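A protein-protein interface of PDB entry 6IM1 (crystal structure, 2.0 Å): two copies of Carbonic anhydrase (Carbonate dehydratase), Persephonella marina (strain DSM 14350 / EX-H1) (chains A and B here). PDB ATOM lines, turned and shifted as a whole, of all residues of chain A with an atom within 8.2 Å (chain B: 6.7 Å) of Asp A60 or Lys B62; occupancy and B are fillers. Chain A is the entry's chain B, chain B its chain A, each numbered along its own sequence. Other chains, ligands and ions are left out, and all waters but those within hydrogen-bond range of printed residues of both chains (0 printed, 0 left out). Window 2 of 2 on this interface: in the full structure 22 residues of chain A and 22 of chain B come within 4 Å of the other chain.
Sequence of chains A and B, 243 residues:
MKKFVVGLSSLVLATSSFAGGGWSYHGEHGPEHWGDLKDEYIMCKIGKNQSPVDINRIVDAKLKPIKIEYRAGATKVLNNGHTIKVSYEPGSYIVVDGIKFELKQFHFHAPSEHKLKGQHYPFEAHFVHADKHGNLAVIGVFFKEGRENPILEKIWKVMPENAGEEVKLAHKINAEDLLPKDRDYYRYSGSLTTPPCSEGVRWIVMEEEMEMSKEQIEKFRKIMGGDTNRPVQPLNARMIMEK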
ATOM      1  N   ARG A  57     -15.680 -34.416   5.234  1.00  0.00           N
ATOM      2  CA  ARG A  57     -14.819 -33.505   5.956  1.00  0.00           C
ATOM      3  C   ARG A  57     -15.770 -32.805   6.898  1.00  0.00           C
ATOM      4  O   ARG A  57     -16.324 -31.810   6.570  1.00  0.00           O
ATOM      5  CB  ARG A  57     -14.130 -32.532   5.015  1.00  0.00           C
ATOM      6  CG  ARG A  57     -13.158 -31.578   5.670  1.00  0.00           C
ATOM      7  CD  ARG A  57     -12.779 -30.470   4.717  1.00  0.00           C
ATOM      8  NE  ARG A  57     -11.782 -30.893   3.800  1.00  0.00           N
ATOM      9  CZ  ARG A  57     -11.545 -30.333   2.639  1.00  0.00           C
ATOM     10  NH1 ARG A  57     -12.253 -29.323   2.217  1.00  0.00           N
ATOM     11  NH2 ARG A  57     -10.590 -30.817   1.909  1.00  0.00           N
ATOM     12  N   ILE A  58     -15.972 -33.358   8.065  1.00  0.00           N
ATOM     13  CA  ILE A  58     -16.944 -32.857   8.990  1.00  0.00           C
ATOM     14  C   ILE A  58     -16.426 -32.398  10.328  1.00  0.00           C
ATOM     15  O   ILE A  58     -15.521 -32.959  10.866  1.00  0.00           O
ATOM     16  CB  ILE A  58     -17.935 -33.984   9.270  1.00  0.00           C
ATOM     17  CG1 ILE A  58     -18.400 -34.608   7.979  1.00  0.00           C
ATOM     18  CG2 ILE A  58     -19.101 -33.511  10.085  1.00  0.00           C
ATOM     19  CD1 ILE A  58     -18.894 -36.003   8.150  1.00  0.00           C
ATOM     20  N   VAL A  59     -17.023 -31.356  10.839  1.00  0.00           N
ATOM     21  CA  VAL A  59     -16.663 -30.837  12.120  1.00  0.00           C
ATOM     22  C   VAL A  59     -17.872 -30.613  13.034  1.00  0.00           C
ATOM     23  O   VAL A  59     -18.858 -30.125  12.598  1.00  0.00           O
ATOM     24  CB  VAL A  59     -15.819 -29.571  11.971  1.00  0.00           C
ATOM     25  CG1 VAL A  59     -16.608 -28.467  11.323  1.00  0.00           C
ATOM     26  CG2 VAL A  59     -15.283 -29.132  13.312  1.00  0.00           C
ATOM     27  N   ASP A  60     -17.789 -30.994  14.293  1.00  0.00           N
ATOM     28  CA  ASP A  60     -18.879 -30.781  15.219  1.00  0.00           C
ATOM     29  C   ASP A  60     -19.055 -29.277  15.378  1.00  0.00           C
ATOM     30  O   ASP A  60     -18.104 -28.580  15.553  1.00  0.00           O
ATOM     31  CB  ASP A  60     -18.559 -31.336  16.613  1.00  0.00           C
ATOM     32  CG  ASP A  60     -18.478 -32.848  16.671  1.00  0.00           C
ATOM     33  OD1 ASP A  60     -18.693 -33.519  15.692  1.00  0.00           O
ATOM     34  OD2 ASP A  60     -18.172 -33.366  17.734  1.00  0.00           O
ATOM     35  N   ALA A  61     -20.275 -28.798  15.333  1.00  0.00           N
ATOM     36  CA  ALA A  61     -20.549 -27.399  15.528  1.00  0.00           C
ATOM     37  C   ALA A  61     -21.785 -27.121  16.396  1.00  0.00           C
ATOM     38  O   ALA A  61     -22.717 -27.846  16.365  1.00  0.00           O
ATOM     39  CB  ALA A  61     -20.643 -26.688  14.208  1.00  0.00           C
ATOM     40  N   LYS A  62     -21.776 -26.029  17.127  1.00  0.00           N
ATOM     41  CA  LYS A  62     -22.878 -25.687  17.980  1.00  0.00           C
ATOM     42  C   LYS A  62     -24.002 -25.013  17.206  1.00  0.00           C
ATOM     43  O   LYS A  62     -24.326 -23.894  17.428  1.00  0.00           O
ATOM     44  CB  LYS A  62     -22.421 -24.770  19.108  1.00  0.00           C
ATOM     45  CG  LYS A  62     -21.734 -25.424  20.252  1.00  0.00           C
ATOM     46  CD  LYS A  62     -21.764 -24.471  21.427  1.00  0.00           C
ATOM     47  CE  LYS A  62     -20.849 -24.924  22.526  1.00  0.00           C
ATOM     48  NZ  LYS A  62     -19.454 -24.964  22.034  1.00  0.00           N
ATOM     49  N   LEU A  63     -24.601 -25.751  16.294  1.00  0.00           N
ATOM     50  CA  LEU A  63     -25.680 -25.255  15.493  1.00  0.00           C
ATOM     51  C   LEU A  63     -27.034 -25.288  16.198  1.00  0.00           C
ATOM     52  O   LEU A  63     -27.269 -26.118  17.008  1.00  0.00           O
ATOM     53  CB  LEU A  63     -25.742 -26.060  14.206  1.00  0.00           C
ATOM     54  CG  LEU A  63     -24.519 -26.012  13.305  1.00  0.00           C
ATOM     55  CD1 LEU A  63     -24.522 -27.114  12.292  1.00  0.00           C
ATOM     56  CD2 LEU A  63     -24.472 -24.690  12.611  1.00  0.00           C
ATOM     57  N   TYR A 186     -26.349 -31.944   8.934  1.00  0.00           N
ATOM     58  CA  TYR A 186     -25.138 -31.399   8.360  1.00  0.00           C
ATOM     59  C   TYR A 186     -25.513 -30.095   7.668  1.00  0.00           C
ATOM     60  O   TYR A 186     -26.573 -30.032   7.012  1.00  0.00           O
ATOM     61  CB  TYR A 186     -24.563 -32.378   7.374  1.00  0.00           C
ATOM     62  CG  TYR A 186     -24.265 -33.748   7.897  1.00  0.00           C
ATOM     63  CD1 TYR A 186     -23.150 -33.950   8.700  1.00  0.00           C
ATOM     64  CD2 TYR A 186     -25.040 -34.856   7.543  1.00  0.00           C
ATOM     65  CE1 TYR A 186     -22.867 -35.228   9.217  1.00  0.00           C
ATOM     66  CE2 TYR A 186     -24.797 -36.119   8.072  1.00  0.00           C
ATOM     67  CZ  TYR A 186     -23.689 -36.298   8.921  1.00  0.00           C
ATOM     68  OH  TYR A 186     -23.382 -37.531   9.372  1.00  0.00           O
ATOM     69  N   GLU A 207     -29.213 -35.886   9.304  1.00  0.00           N
ATOM     70  CA  GLU A 207     -28.309 -36.958   9.630  1.00  0.00           C
ATOM     71  C   GLU A 207     -29.059 -38.314   9.655  1.00  0.00           C
ATOM     72  O   GLU A 207     -28.471 -39.363   9.328  1.00  0.00           O
ATOM     73  CB  GLU A 207     -27.677 -36.686  11.032  1.00  0.00           C
ATOM     74  CG  GLU A 207     -26.646 -37.723  11.460  1.00  0.00           C
ATOM     75  CD  GLU A 207     -26.244 -37.624  12.945  1.00  0.00           C
ATOM     76  OE1 GLU A 207     -27.128 -37.778  13.851  1.00  0.00           O
ATOM     77  OE2 GLU A 207     -25.039 -37.411  13.216  1.00  0.00           O
ATOM     78  N   MET A 239     -15.900 -26.800   4.729  1.00  0.00           N
ATOM     79  CA  MET A 239     -16.112 -27.880   5.700  1.00  0.00           C
ATOM     80  C   MET A 239     -17.600 -28.110   5.867  1.00  0.00           C
ATOM     81  O   MET A 239     -18.383 -27.276   5.519  1.00  0.00           O
ATOM     82  CB  MET A 239     -15.607 -27.419   7.062  1.00  0.00           C
ATOM     83  CG  MET A 239     -14.158 -27.110   7.026  1.00  0.00           C
ATOM     84  SD  MET A 239     -13.417 -27.426   8.624  1.00  0.00           S
ATOM     85  CE  MET A 239     -13.633 -29.233   8.536  1.00  0.00           C
ATOM     86  N   ILE A 240     -17.993 -29.314   6.245  1.00  0.00           N
ATOM     87  CA  ILE A 240     -19.400 -29.563   6.497  1.00  0.00           C
ATOM     88  C   ILE A 240     -19.538 -29.482   8.054  1.00  0.00           C
ATOM     89  O   ILE A 240     -18.713 -30.105   8.763  1.00  0.00           O
ATOM     90  CB  ILE A 240     -19.792 -30.943   6.014  1.00  0.00           C
ATOM     91  CG1 ILE A 240     -19.351 -31.281   4.582  1.00  0.00           C
ATOM     92  CG2 ILE A 240     -21.267 -31.130   6.282  1.00  0.00           C
ATOM     93  CD1 ILE A 240     -19.873 -30.326   3.657  1.00  0.00           C
ATOM     94  N   MET A 241     -20.470 -28.724   8.551  1.00  0.00           N
ATOM     95  CA  MET A 241     -20.708 -28.620   9.981  1.00  0.00           C
ATOM     96  C   MET A 241     -21.779 -29.612  10.369  1.00  0.00           C
ATOM     97  O   MET A 241     -22.768 -29.797   9.619  1.00  0.00           O
ATOM     98  CB  MET A 241     -21.204 -27.231  10.300  1.00  0.00           C
ATOM     99  CG  MET A 241     -20.113 -26.196  10.028  1.00  0.00           C
ATOM    100  SD  MET A 241     -20.778 -24.522  10.161  1.00  0.00           S
ATOM    101  CE  MET A 241     -21.974 -24.454   8.804  1.00  0.00           C
ATOM    102  N   GLU A 242     -21.603 -30.249  11.509  1.00  0.00           N
ATOM    103  CA  GLU A 242     -22.608 -31.186  12.042  1.00  0.00           C
ATOM    104  C   GLU A 242     -23.149 -30.755  13.358  1.00  0.00           C
ATOM    105  O   GLU A 242     -22.351 -30.514  14.293  1.00  0.00           O
ATOM    106  CB  GLU A 242     -21.956 -32.574  12.189  1.00  0.00           C
ATOM    107  CG  GLU A 242     -22.940 -33.635  12.652  1.00  0.00           C
ATOM    108  CD  GLU A 242     -22.274 -34.930  13.140  1.00  0.00           C
ATOM    109  OE1 GLU A 242     -21.059 -35.178  12.842  1.00  0.00           O
ATOM    110  OE2 GLU A 242     -22.949 -35.598  13.910  1.00  0.00           O
ATOM    111  N   LYS A 243     -24.471 -30.707  13.474  1.00  0.00           N
ATOM    112  CA  LYS A 243     -25.127 -30.380  14.760  1.00  0.00           C
ATOM    113  C   LYS A 243     -25.000 -31.387  16.014  1.00  0.00           C
ATOM    114  O   LYS A 243     -24.955 -32.576  15.739  1.00  0.00           O
ATOM    115  CB  LYS A 243     -26.552 -30.101  14.510  1.00  0.00           C
ATOM    116  CG  LYS A 243     -27.285 -29.716  15.800  1.00  0.00           C
ATOM    117  CD  LYS A 243     -28.727 -29.471  15.586  1.00  0.00           C
ATOM    118  CE  LYS A 243     -29.389 -28.866  16.819  1.00  0.00           C
ATOM    119  NZ  LYS A 243     -29.582 -29.903  17.828  1.00  0.00           N
ATOM    120  N   ASP B  60     -19.482 -21.839  17.253  1.00  0.00           N
ATOM    121  CA  ASP B  60     -18.391 -22.618  17.803  1.00  0.00           C
ATOM    122  C   ASP B  60     -18.239 -23.922  17.061  1.00  0.00           C
ATOM    123  O   ASP B  60     -19.228 -24.621  16.806  1.00  0.00           O
ATOM    124  CB  ASP B  60     -18.620 -23.043  19.274  1.00  0.00           C
ATOM    125  CG  ASP B  60     -18.663 -21.844  20.265  1.00  0.00           C
ATOM    126  OD1 ASP B  60     -18.483 -20.700  19.869  1.00  0.00           O
ATOM    127  OD2 ASP B  60     -18.883 -22.101  21.470  1.00  0.00           O
ATOM    128  N   ALA B  61     -17.016 -24.299  16.765  1.00  0.00           N
ATOM    129  CA  ALA B  61     -16.768 -25.533  16.059  1.00  0.00           C
ATOM    130  C   ALA B  61     -15.541 -26.211  16.557  1.00  0.00           C
ATOM    131  O   ALA B  61     -14.564 -25.530  16.864  1.00  0.00           O
ATOM    132  CB  ALA B  61     -16.691 -25.284  14.536  1.00  0.00           C
ATOM    133  N   LYS B  62     -15.501 -27.514  16.479  1.00  0.00           N
ATOM    134  CA  LYS B  62     -14.354 -28.287  16.946  1.00  0.00           C
ATOM    135  C   LYS B  62     -13.236 -28.323  15.900  1.00  0.00           C
ATOM    136  O   LYS B  62     -12.939 -29.343  15.401  1.00  0.00           O
ATOM    137  CB  LYS B  62     -14.737 -29.698  17.273  1.00  0.00           C
ATOM    138  CG  LYS B  62     -15.529 -29.842  18.535  1.00  0.00           C
ATOM    139  CD  LYS B  62     -15.498 -31.348  18.975  1.00  0.00           C
ATOM    140  CE  LYS B  62     -16.387 -31.663  20.177  1.00  0.00           C
ATOM    141  NZ  LYS B  62     -17.846 -31.501  19.929  1.00  0.00           N
ATOM    142  N   LEU B  63     -12.709 -27.169  15.552  1.00  0.00           N
ATOM    143  CA  LEU B  63     -11.664 -27.071  14.563  1.00  0.00           C
ATOM    144  C   LEU B  63     -10.302 -27.515  15.058  1.00  0.00           C
ATOM    145  O   LEU B  63     -10.013 -27.378  16.196  1.00  0.00           O
ATOM    146  CB  LEU B  63     -11.573 -25.653  14.037  1.00  0.00           C
ATOM    147  CG  LEU B  63     -12.845 -25.132  13.388  1.00  0.00           C
ATOM    148  CD1 LEU B  63     -12.843 -23.649  13.161  1.00  0.00           C
ATOM    149  CD2 LEU B  63     -13.133 -25.865  12.114  1.00  0.00           C
ATOM    150  N   LYS B  64      -9.487 -28.031  14.171  1.00  0.00           N
ATOM    151  CA  LYS B  64      -8.145 -28.417  14.503  1.00  0.00           C
ATOM    152  C   LYS B  64      -7.220 -27.215  14.505  1.00  0.00           C
ATOM    153  O   LYS B  64      -7.423 -26.284  13.791  1.00  0.00           O
ATOM    154  CB  LYS B  64      -7.565 -29.396  13.487  1.00  0.00           C
ATOM    155  CG  LYS B  64      -8.227 -30.727  13.340  1.00  0.00           C
ATOM    156  CD  LYS B  64      -7.264 -31.646  12.627  1.00  0.00           C
ATOM    157  CE  LYS B  64      -6.051 -31.815  13.511  1.00  0.00           C
ATOM    158  NZ  LYS B  64      -4.941 -32.655  13.005  1.00  0.00           N
ATOM    159  N   GLU B 242     -15.788 -20.795  14.415  1.00  0.00           N
ATOM    160  CA  GLU B 242     -14.776 -20.334  15.366  1.00  0.00           C
ATOM    161  C   GLU B 242     -14.198 -21.495  16.146  1.00  0.00           C
ATOM    162  O   GLU B 242     -14.946 -22.239  16.804  1.00  0.00           O
ATOM    163  CB  GLU B 242     -15.382 -19.375  16.343  1.00  0.00           C
ATOM    164  CG  GLU B 242     -14.392 -18.764  17.286  1.00  0.00           C
ATOM    165  CD  GLU B 242     -15.034 -18.014  18.470  1.00  0.00           C
ATOM    166  OE1 GLU B 242     -16.244 -17.656  18.437  1.00  0.00           O
ATOM    167  OE2 GLU B 242     -14.247 -17.832  19.442  1.00  0.00           O
ATOM    168  N   LYS B 243     -12.867 -21.544  16.200  1.00  0.00           N
ATOM    169  CA  LYS B 243     -12.157 -22.593  17.030  1.00  0.00           C
ATOM    170  C   LYS B 243     -12.226 -22.499  18.625  1.00  0.00           C
ATOM    171  O   LYS B 243     -12.256 -21.363  19.108  1.00  0.00           O
ATOM    172  CB  LYS B 243     -10.739 -22.658  16.615  1.00  0.00           C
ATOM    173  CG  LYS B 243      -9.970 -23.712  17.419  1.00  0.00           C
ATOM    174  CD  LYS B 243      -8.533 -23.788  17.049  1.00  0.00           C
ATOM    175  CE  LYS B 243      -7.858 -25.008  17.660  1.00  0.00           C
ATOM    176  NZ  LYS B 243      -7.640 -24.770  19.083  1.00  0.00           N
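The backbone carbonyl oxygen (O) of Asp B60 sits at hydrogen-bond distance from the backbone NH (N) of Lys A62, 2.9 Å away. The backbone NH (N) of Lys B62 lies within hydrogen-bond range of the backbone carbonyl oxygen (O) of Asp A60 (3.0 Å).
The backbone NH (N) of Ala B61 is in hydrogen-bond range of the backbone carbonyl oxygen (O) of Glu B242, 2.9 Å away. N of Val A59 sits at hydrogen-bond distance from O of Ile A240 (3.0 Å). N of Glu A242 sits at hydrogen-bond distance from O of Val A59, 3.0 Å away. The backbone carbonyl oxygen (O) of Glu A242 is in hydrogen-bond range of the backbone NH (N) of Ala A61, at 2.9 Å.
Among the printed residues, merely in contact across the chains: Val A59 with Lys B62 (3.1 Å), Ala A61 with Asp B60 (3.3 Å), Asp A60 with Ala B61 (3.4 Å), Met A239 with Leu B63 (3.8 Å) and Val A59 with Leu B63 (3.9 Å).
Asp A60 touches just these residues of chain B: Ala B61 and Lys B62. Of chain A, only Val A59 and Asp A60 come within 4 Å of Lys B62. Of chain A, only Asp A60 (3.4 Å) comes within 4 Å of Ala B61. Printed residues of chain B within 4 Å of Met A239: Leu B63. Printed residues of chain B within 4 Å of Ala A61: Asp B60. Of the printed residues of chain A, Asp B60 touches Ala A61 (3.3 Å) and Lys A62 (2.9 Å). Of the printed residues of chain B, Lys A62 touches Asp B60 (2.9 Å). Printed residues of chain A within 4 Å of Leu B63: Val A59 and Met A239. Glu A207 touches none of the printed residues of chain B.
Of the 7 printed residues of chain B, 4 touch a printed residue of chain A. Of the 14 printed residues of chain A, 5 touch a printed residue of chain B. Hydrophobic or aromatic side chains of chain A within 4 Å of the printed part of chain B: Val A59, Ala A61 and Met A239.
Asp A60 touches Ala B61, and with the chains exchanged Ala A61 touches Asp B60. Asp A60 touches Lys B62, and with the chains exchanged Lys A62 touches Asp B60. Of the 7 pairs that touch across the chains among the printed residues, 4 have their exchanged pair printed and touching as well.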
